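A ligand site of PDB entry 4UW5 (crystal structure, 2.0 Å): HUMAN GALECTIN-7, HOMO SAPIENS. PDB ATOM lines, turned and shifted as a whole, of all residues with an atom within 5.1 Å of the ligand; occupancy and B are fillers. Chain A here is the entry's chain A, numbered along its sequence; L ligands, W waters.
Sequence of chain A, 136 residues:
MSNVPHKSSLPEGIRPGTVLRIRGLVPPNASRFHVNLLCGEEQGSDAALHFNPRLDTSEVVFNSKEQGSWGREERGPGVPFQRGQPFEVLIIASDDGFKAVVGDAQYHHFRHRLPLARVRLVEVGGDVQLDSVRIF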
ATOM      1  N   ARG A  32     -39.371 -31.309  14.394  1.00  0.00           N
ATOM      2  CA  ARG A  32     -39.372 -30.483  15.595  1.00  0.00           C
ATOM      3  C   ARG A  32     -40.700 -29.789  15.850  1.00  0.00           C
ATOM      4  O   ARG A  32     -41.467 -29.526  14.925  1.00  0.00           O
ATOM      5  CB  ARG A  32     -38.260 -29.441  15.512  1.00  0.00           C
ATOM      6  CG  ARG A  32     -38.155 -28.700  14.173  1.00  0.00           C
ATOM      7  CD  ARG A  32     -36.909 -27.803  14.161  1.00  0.00           C
ATOM      8  NE  ARG A  32     -35.667 -28.574  14.198  1.00  0.00           N
ATOM      9  CZ  ARG A  32     -34.450 -28.035  14.242  1.00  0.00           C
ATOM     10  NH1 ARG A  32     -34.282 -26.714  14.302  1.00  0.00           N
ATOM     11  NH2 ARG A  32     -33.371 -28.817  14.251  1.00  0.00           N
ATOM     12  N   HIS A  50     -38.903 -19.949  24.715  1.00  0.00           N
ATOM     13  CA  HIS A  50     -39.021 -20.694  23.469  1.00  0.00           C
ATOM     14  C   HIS A  50     -38.557 -22.090  23.806  1.00  0.00           C
ATOM     15  O   HIS A  50     -37.443 -22.271  24.255  1.00  0.00           O
ATOM     16  CB  HIS A  50     -38.189 -20.044  22.343  1.00  0.00           C
ATOM     17  CG  HIS A  50     -37.970 -20.907  21.138  1.00  0.00           C
ATOM     18  ND1 HIS A  50     -38.940 -21.093  20.165  1.00  0.00           N
ATOM     19  CD2 HIS A  50     -36.879 -21.589  20.708  1.00  0.00           C
ATOM     20  CE1 HIS A  50     -38.450 -21.869  19.204  1.00  0.00           C
ATOM     21  NE2 HIS A  50     -37.202 -22.183  19.516  1.00  0.00           N
ATOM     22  N   ASN A  52     -38.254 -26.028  22.493  1.00  0.00           N
ATOM     23  CA  ASN A  52     -38.128 -26.514  21.117  1.00  0.00           C
ATOM     24  C   ASN A  52     -37.532 -27.901  21.048  1.00  0.00           C
ATOM     25  O   ASN A  52     -36.336 -28.045  20.875  1.00  0.00           O
ATOM     26  CB  ASN A  52     -37.296 -25.509  20.298  1.00  0.00           C
ATOM     27  CG  ASN A  52     -37.169 -25.868  18.805  1.00  0.00           C
ATOM     28  OD1 ASN A  52     -36.234 -25.430  18.155  1.00  0.00           O
ATOM     29  ND2 ASN A  52     -38.106 -26.641  18.277  1.00  0.00           N
ATOM     30  N   ARG A  54     -36.436 -31.173  19.493  1.00  0.00           N
ATOM     31  CA  ARG A  54     -35.981 -31.389  18.125  1.00  0.00           C
ATOM     32  C   ARG A  54     -35.674 -32.853  17.928  1.00  0.00           C
ATOM     33  O   ARG A  54     -34.629 -33.334  18.361  1.00  0.00           O
ATOM     34  CB  ARG A  54     -34.766 -30.538  17.824  1.00  0.00           C
ATOM     35  CG  ARG A  54     -35.018 -29.055  17.883  1.00  0.00           C
ATOM     36  CD  ARG A  54     -33.751 -28.291  17.597  1.00  0.00           C
ATOM     37  NE  ARG A  54     -33.883 -26.842  17.666  1.00  0.00           N
ATOM     38  CZ  ARG A  54     -32.857 -26.021  17.534  1.00  0.00           C
ATOM     39  NH1 ARG A  54     -31.626 -26.521  17.368  1.00  0.00           N
ATOM     40  NH2 ARG A  54     -33.024 -24.712  17.614  1.00  0.00           N
ATOM     41  N   THR A  57     -32.439 -33.563  15.506  1.00  0.00           N
ATOM     42  CA  THR A  57     -31.085 -33.450  16.062  1.00  0.00           C
ATOM     43  C   THR A  57     -30.974 -33.935  17.514  1.00  0.00           C
ATOM     44  O   THR A  57     -29.963 -33.700  18.171  1.00  0.00           O
ATOM     45  CB  THR A  57     -30.557 -32.010  15.979  1.00  0.00           C
ATOM     46  OG1 THR A  57     -31.522 -31.088  16.513  1.00  0.00           O
ATOM     47  CG2 THR A  57     -30.292 -31.635  14.533  1.00  0.00           C
ATOM     48  N   GLU A  59     -32.304 -33.195  20.555  1.00  0.00           N
ATOM     49  CA  GLU A  59     -32.046 -32.194  21.583  1.00  0.00           C
ATOM     50  C   GLU A  59     -33.343 -31.489  21.952  1.00  0.00           C
ATOM     51  O   GLU A  59     -34.359 -31.620  21.270  1.00  0.00           O
ATOM     52  CB  GLU A  59     -30.989 -31.176  21.095  1.00  0.00           C
ATOM     53  CG  GLU A  59     -31.264 -30.638  19.695  1.00  0.00           C
ATOM     54  CD  GLU A  59     -30.275 -29.560  19.190  1.00  0.00           C
ATOM     55  OE1 GLU A  59     -29.423 -29.080  19.964  1.00  0.00           O
ATOM     56  OE2 GLU A  59     -30.373 -29.191  17.986  1.00  0.00           O
ATOM     57  N   VAL A  61     -33.982 -27.488  22.891  1.00  0.00           N
ATOM     58  CA  VAL A  61     -33.355 -26.203  23.206  1.00  0.00           C
ATOM     59  C   VAL A  61     -34.336 -25.226  23.855  1.00  0.00           C
ATOM     60  O   VAL A  61     -35.532 -25.272  23.601  1.00  0.00           O
ATOM     61  CB  VAL A  61     -32.688 -25.587  21.936  1.00  0.00           C
ATOM     62  CG1 VAL A  61     -32.951 -26.444  20.726  1.00  0.00           C
ATOM     63  CG2 VAL A  61     -33.114 -24.169  21.708  1.00  0.00           C
ATOM     64  N   ASN A  63     -34.638 -20.994  24.776  1.00  0.00           N
ATOM     65  CA  ASN A  63     -34.075 -19.687  24.492  1.00  0.00           C
ATOM     66  C   ASN A  63     -35.122 -18.613  24.646  1.00  0.00           C
ATOM     67  O   ASN A  63     -36.300 -18.917  24.789  1.00  0.00           O
ATOM     68  CB  ASN A  63     -33.473 -19.632  23.067  1.00  0.00           C
ATOM     69  CG  ASN A  63     -32.282 -18.719  22.990  1.00  0.00           C
ATOM     70  OD1 ASN A  63     -32.025 -17.921  23.886  1.00  0.00           O
ATOM     71  ND2 ASN A  63     -31.532 -18.828  21.903  1.00  0.00           N
ATOM     72  N   TRP A  70     -32.114 -13.882  18.991  1.00  0.00           N
ATOM     73  CA  TRP A  70     -32.060 -14.993  19.945  1.00  0.00           C
ATOM     74  C   TRP A  70     -30.951 -14.784  20.970  1.00  0.00           C
ATOM     75  O   TRP A  70     -29.892 -14.247  20.637  1.00  0.00           O
ATOM     76  CB  TRP A  70     -31.845 -16.330  19.237  1.00  0.00           C
ATOM     77  CG  TRP A  70     -32.963 -16.753  18.351  1.00  0.00           C
ATOM     78  CD1 TRP A  70     -32.945 -16.775  16.981  1.00  0.00           C
ATOM     79  CD2 TRP A  70     -34.265 -17.221  18.750  1.00  0.00           C
ATOM     80  NE1 TRP A  70     -34.165 -17.221  16.501  1.00  0.00           N
ATOM     81  CE2 TRP A  70     -34.985 -17.503  17.564  1.00  0.00           C
ATOM     82  CE3 TRP A  70     -34.893 -17.424  19.989  1.00  0.00           C
ATOM     83  CZ2 TRP A  70     -36.302 -17.968  17.592  1.00  0.00           C
ATOM     84  CZ3 TRP A  70     -36.197 -17.892  20.010  1.00  0.00           C
ATOM     85  CH2 TRP A  70     -36.889 -18.165  18.828  1.00  0.00           C
ATOM     86  N   GLU A  73     -28.580 -20.063  24.022  1.00  0.00           N
ATOM     87  CA  GLU A  73     -29.349 -21.288  24.125  1.00  0.00           C
ATOM     88  C   GLU A  73     -28.994 -22.030  25.394  1.00  0.00           C
ATOM     89  O   GLU A  73     -27.820 -22.075  25.785  1.00  0.00           O
ATOM     90  CB  GLU A  73     -29.099 -22.207  22.910  1.00  0.00           C
ATOM     91  CG  GLU A  73     -29.502 -21.634  21.563  1.00  0.00           C
ATOM     92  CD  GLU A  73     -29.386 -22.642  20.428  1.00  0.00           C
ATOM     93  OE1 GLU A  73     -28.569 -23.586  20.523  1.00  0.00           O
ATOM     94  OE2 GLU A  73     -30.120 -22.499  19.447  1.00  0.00           O
ATOM     95  N   ARG A  75     -29.803 -26.067  26.885  1.00  0.00           N
ATOM     96  CA  ARG A  75     -30.280 -27.374  26.431  1.00  0.00           C
ATOM     97  C   ARG A  75     -30.550 -28.239  27.651  1.00  0.00           C
ATOM     98  O   ARG A  75     -29.934 -28.052  28.694  1.00  0.00           O
ATOM     99  CB  ARG A  75     -29.253 -28.072  25.527  1.00  0.00           C
ATOM    100  CG  ARG A  75     -29.266 -27.563  24.111  1.00  0.00           C
ATOM    101  CD  ARG A  75     -28.149 -28.151  23.269  1.00  0.00           C
ATOM    102  NE  ARG A  75     -28.378 -27.852  21.861  1.00  0.00           N
ATOM    103  CZ  ARG A  75     -28.171 -26.667  21.311  1.00  0.00           C
ATOM    104  NH1 ARG A  75     -27.723 -25.642  22.038  1.00  0.00           N
ATOM    105  NH2 ARG A  75     -28.405 -26.504  20.017  1.00  0.00           N
HETATM  106  O1  LIG L   1     -22.064 -24.508  16.673  1.00  0.00           O
HETATM  107  C1  LIG L   1     -22.705 -25.706  16.215  1.00  0.00           C
HETATM  108  C2  LIG L   1     -22.332 -23.456  15.726  1.00  0.00           C
HETATM  109  C3  LIG L   1     -23.740 -22.909  15.971  1.00  0.00           C
HETATM  110  C4  LIG L   1     -24.873 -23.320  15.424  1.00  0.00           C
HETATM  111  N1  LIG L   1     -24.011 -21.915  16.816  1.00  0.00           N
HETATM  112  N2  LIG L   1     -25.180 -21.726  16.788  1.00  0.00           N
HETATM  113  N3  LIG L   1     -25.771 -22.512  15.996  1.00  0.00           N
HETATM  114  C5  LIG L   1     -27.241 -22.358  15.922  1.00  0.00           C
HETATM  115  C6  LIG L   1     -28.005 -23.664  16.165  1.00  0.00           C
HETATM  116  O2  LIG L   1     -27.455 -24.349  17.252  1.00  0.00           O
HETATM  117  C7  LIG L   1     -29.434 -23.250  16.506  1.00  0.00           C
HETATM  118  O3  LIG L   1     -30.244 -24.356  16.881  1.00  0.00           O
HETATM  119  O4  LIG L   1     -27.753 -21.729  14.761  1.00  0.00           O
HETATM  120  C8  LIG L   1     -29.145 -21.365  15.008  1.00  0.00           C
HETATM  121  C9  LIG L   1     -29.631 -20.590  13.800  1.00  0.00           C
HETATM  122  O5  LIG L   1     -29.929 -19.293  14.320  1.00  0.00           O
HETATM  123  C10 LIG L   1     -29.963 -22.631  15.269  1.00  0.00           C
HETATM  124  O6  LIG L   1     -31.425 -22.534  15.330  1.00  0.00           O
HETATM  125  C11 LIG L   1     -32.277 -21.531  15.918  1.00  0.00           C
HETATM  126  O7  LIG L   1     -32.394 -21.673  17.344  1.00  0.00           O
HETATM  127  C12 LIG L   1     -33.396 -20.797  17.919  1.00  0.00           C
HETATM  128  C13 LIG L   1     -33.308 -20.911  19.427  1.00  0.00           C
HETATM  129  O8  LIG L   1     -31.935 -20.744  19.826  1.00  0.00           O
HETATM  130  C14 LIG L   1     -34.758 -21.186  17.423  1.00  0.00           C
HETATM  131  O9  LIG L   1     -35.056 -22.566  17.717  1.00  0.00           O
HETATM  132  C15 LIG L   1     -34.744 -20.969  15.925  1.00  0.00           C
HETATM  133  O10 LIG L   1     -35.950 -21.397  15.354  1.00  0.00           O
HETATM  134  C16 LIG L   1     -33.620 -21.824  15.306  1.00  0.00           C
HETATM  135  O11 LIG L   1     -33.554 -21.550  13.898  1.00  0.00           O
HETATM  136  C17 LIG L   1     -22.584 -26.822  17.252  1.00  0.00           C
HETATM  137  C18 LIG L   1     -21.330 -27.642  16.929  1.00  0.00           C
HETATM  138  O12 LIG L   1     -20.212 -26.779  16.999  1.00  0.00           O
HETATM  139  C19 LIG L   1     -18.962 -27.354  16.560  1.00  0.00           C
HETATM  140  C20 LIG L   1     -17.977 -26.974  17.645  1.00  0.00           C
HETATM  141  C21 LIG L   1     -17.465 -27.825  18.516  1.00  0.00           C
HETATM  142  N4  LIG L   1     -17.573 -25.758  17.939  1.00  0.00           N
HETATM  143  N5  LIG L   1     -16.804 -25.852  18.933  1.00  0.00           N
HETATM  144  N6  LIG L   1     -16.724 -27.053  19.292  1.00  0.00           N
HETATM  145  C22 LIG L   1     -16.005 -27.769  20.357  1.00  0.00           C
HETATM  146  C23 LIG L   1     -16.077 -27.121  21.734  1.00  0.00           C
HETATM  147  O13 LIG L   1     -17.404 -26.801  22.110  1.00  0.00           O
HETATM  148  C24 LIG L   1     -15.520 -28.142  22.722  1.00  0.00           C
HETATM  149  O14 LIG L   1     -15.718 -27.709  24.078  1.00  0.00           O
HETATM  150  O15 LIG L   1     -14.661 -27.994  20.019  1.00  0.00           O
HETATM  151  C25 LIG L   1     -14.040 -28.900  20.936  1.00  0.00           C
HETATM  152  C26 LIG L   1     -12.673 -29.088  20.361  1.00  0.00           C
HETATM  153  O16 LIG L   1     -12.846 -29.792  19.133  1.00  0.00           O
HETATM  154  C27 LIG L   1     -14.066 -28.260  22.342  1.00  0.00           C
HETATM  155  O17 LIG L   1     -13.266 -28.893  23.370  1.00  0.00           O
HETATM  156  C28 LIG L   1     -13.079 -30.280  23.581  1.00  0.00           C
HETATM  157  O18 LIG L   1     -14.216 -30.891  24.187  1.00  0.00           O
HETATM  158  C29 LIG L   1     -13.948 -32.237  24.673  1.00  0.00           C
HETATM  159  C30 LIG L   1     -15.222 -32.764  25.337  1.00  0.00           C
HETATM  160  O19 LIG L   1     -16.213 -32.955  24.310  1.00  0.00           O
HETATM  161  C31 LIG L   1     -12.752 -32.266  25.675  1.00  0.00           C
HETATM  162  O20 LIG L   1     -13.020 -31.438  26.785  1.00  0.00           O
HETATM  163  C32 LIG L   1     -11.530 -31.680  24.979  1.00  0.00           C
HETATM  164  O21 LIG L   1     -10.415 -31.554  25.912  1.00  0.00           O
HETATM  165  C33 LIG L   1     -11.889 -30.294  24.551  1.00  0.00           C
HETATM  166  O22 LIG L   1     -10.761 -29.670  23.922  1.00  0.00           O
HETATM  167  N7  LIG L   1     -22.499 -26.230  18.596  1.00  0.00           N
HETATM  168  C34 LIG L   1     -23.786 -27.749  17.143  1.00  0.00           C
HETATM  169  O23 LIG L   1     -24.793 -27.163  16.316  1.00  0.00           O
HETATM  170  C35 LIG L   1     -26.049 -27.843  16.525  1.00  0.00           C
HETATM  171  C36 LIG L   1     -25.911 -29.290  16.093  1.00  0.00           C
HETATM  172  C37 LIG L   1     -26.420 -30.378  16.645  1.00  0.00           C
HETATM  173  N8  LIG L   1     -25.206 -29.665  15.053  1.00  0.00           N
HETATM  174  N9  LIG L   1     -25.271 -30.821  14.961  1.00  0.00           N
HETATM  175  N10 LIG L   1     -25.959 -31.315  15.827  1.00  0.00           N
HETATM  176  C38 LIG L   1     -26.000 -32.759  15.674  1.00  0.00           C
HETATM  177  C39 LIG L   1     -24.687 -33.357  16.219  1.00  0.00           C
HETATM  178  O24 LIG L   1     -24.544 -33.131  17.633  1.00  0.00           O
HETATM  179  C40 LIG L   1     -24.648 -34.831  15.906  1.00  0.00           C
HETATM  180  O25 LIG L   1     -23.452 -35.420  16.503  1.00  0.00           O
HETATM  181  O26 LIG L   1     -25.983 -32.883  14.238  1.00  0.00           O
HETATM  182  C41 LIG L   1     -25.881 -34.245  13.809  1.00  0.00           C
HETATM  183  C42 LIG L   1     -25.797 -34.139  12.306  1.00  0.00           C
HETATM  184  O27 LIG L   1     -26.027 -35.424  11.784  1.00  0.00           O
HETATM  185  C43 LIG L   1     -24.617 -34.943  14.368  1.00  0.00           C
HETATM  186  O28 LIG L   1     -24.566 -36.340  13.965  1.00  0.00           O
HETATM  187  C44 LIG L   1     -23.214 -36.774  13.643  1.00  0.00           C
HETATM  188  O29 LIG L   1     -22.725 -36.025  12.502  1.00  0.00           O
HETATM  189  C45 LIG L   1     -21.371 -36.320  12.121  1.00  0.00           C
HETATM  190  C46 LIG L   1     -20.967 -35.410  10.933  1.00  0.00           C
HETATM  191  O30 LIG L   1     -20.681 -34.048  11.373  1.00  0.00           O
HETATM  192  C47 LIG L   1     -21.241 -37.827  11.762  1.00  0.00           C
HETATM  193  O31 LIG L   1     -21.997 -38.144  10.588  1.00  0.00           O
HETATM  194  C48 LIG L   1     -21.774 -38.676  12.940  1.00  0.00           C
HETATM  195  O32 LIG L   1     -21.843 -40.049  12.580  1.00  0.00           O
HETATM  196  C49 LIG L   1     -23.204 -38.241  13.285  1.00  0.00           C
HETATM  197  O33 LIG L   1     -23.638 -39.036  14.395  1.00  0.00           O
HETATM  198  O   HOH W   1     -36.750 -24.077  15.904  1.00  0.00           O
HETATM  199  O   HOH W   2     -30.096 -19.108  18.317  1.00  0.00           O
HETATM  200  O   HOH W   3     -30.767 -17.019  14.062  1.00  0.00           O
HETATM  201  O   HOH W   4     -21.421 -33.447  14.371  1.00  0.00           O
HETATM  202  O   HOH W   5      -8.459 -32.382  23.452  1.00  0.00           O
HETATM  203  O   HOH W   6     -12.007 -26.541  24.044  1.00  0.00           O
HETATM  204  O   HOH W   7     -31.842 -24.836  13.598  1.00  0.00           O
HETATM  205  O   HOH W   8     -10.513 -29.892  28.221  1.00  0.00           O
HETATM  206  O   HOH W   9     -33.539 -18.320  13.505  1.00  0.00           O
HETATM  207  O   HOH W  10     -36.804 -20.059  12.901  1.00  0.00           O
HETATM  208  O   HOH W  11      -8.587 -33.490  25.889  1.00  0.00           O
HETATM  209  O   HOH W  12     -20.725 -34.159  17.707  1.00  0.00           O
HETATM  210  O   HOH W  13     -10.488 -30.982  21.916  1.00  0.00           O
HETATM  211  O   HOH W  14     -18.338 -22.761  17.685  1.00  0.00           O
HETATM  212  O   HOH W  15     -25.943 -20.226  13.179  1.00  0.00           O
HETATM  213  O   HOH W  16     -20.832 -27.383  20.294  1.00  0.00           O
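The side-chain amide nitrogen (ND2) of Asn 63 sits at hydrogen-bond distance from an oxygen (O8) of the ligand (2.9 Å). NH1 of Arg 54 is in hydrogen-bond range of O3 of the ligand, at 2.6 Å. OD1 of Asn 52 sits at hydrogen-bond distance from O9 of the ligand (3.1 Å). The side-chain carboxylate (OE2) of Glu 73 sits at hydrogen-bond distance from an oxygen (O8) of the ligand. A ring nitrogen (NE2) of His 50 lies within hydrogen-bond range of an oxygen (O9) of the ligand (2.8 Å).
Residues that only touch the ligand: Val 61 (3.98 Å), Trp 70 (3.6 Å) and Arg 75 (3.6 Å). Hydrophobic or aromatic side chains within 4 Å of the ligand: His 50, Val 61 and Trp 70. Of the 11 residues printed, 8 come within 4 Å of the ligand.
Water W1 bridges the side-chain amide oxygen of Asn 52 (2.7 Å) and an oxygen (O10) of the ligand (2.9 Å). Water W7 lies within hydrogen-bond range of an oxygen (O6) of the ligand (2.9 Å) and the guanidinium group of Arg 32 (3.2 Å). Water W9 lies within hydrogen-bond range of the indole nitrogen of Trp 70 and an oxygen (O11) of the ligand.
NE of Arg 75 is in salt-bridge range of OE1 of Glu 59 (2.5 Å). The backbone NH (N) of His 50 is in hydrogen-bond range of the backbone carbonyl oxygen (O) of Asn 63 (2.8 Å). NE of Arg 54 is in hydrogen-bond range of OD1 of Asn 52, 2.8 Å away. The backbone carbonyl oxygen (O) of Val 61 lies within hydrogen-bond range of the backbone NH (N) of Asn 52. The side-chain carboxylate of Glu 59 is in salt-bridge range of the guanidinium group of Arg 54 (3.0 Å). NH1 of Arg 75 lies within salt-bridge range of OE1 of Glu 73, at 2.7 Å.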
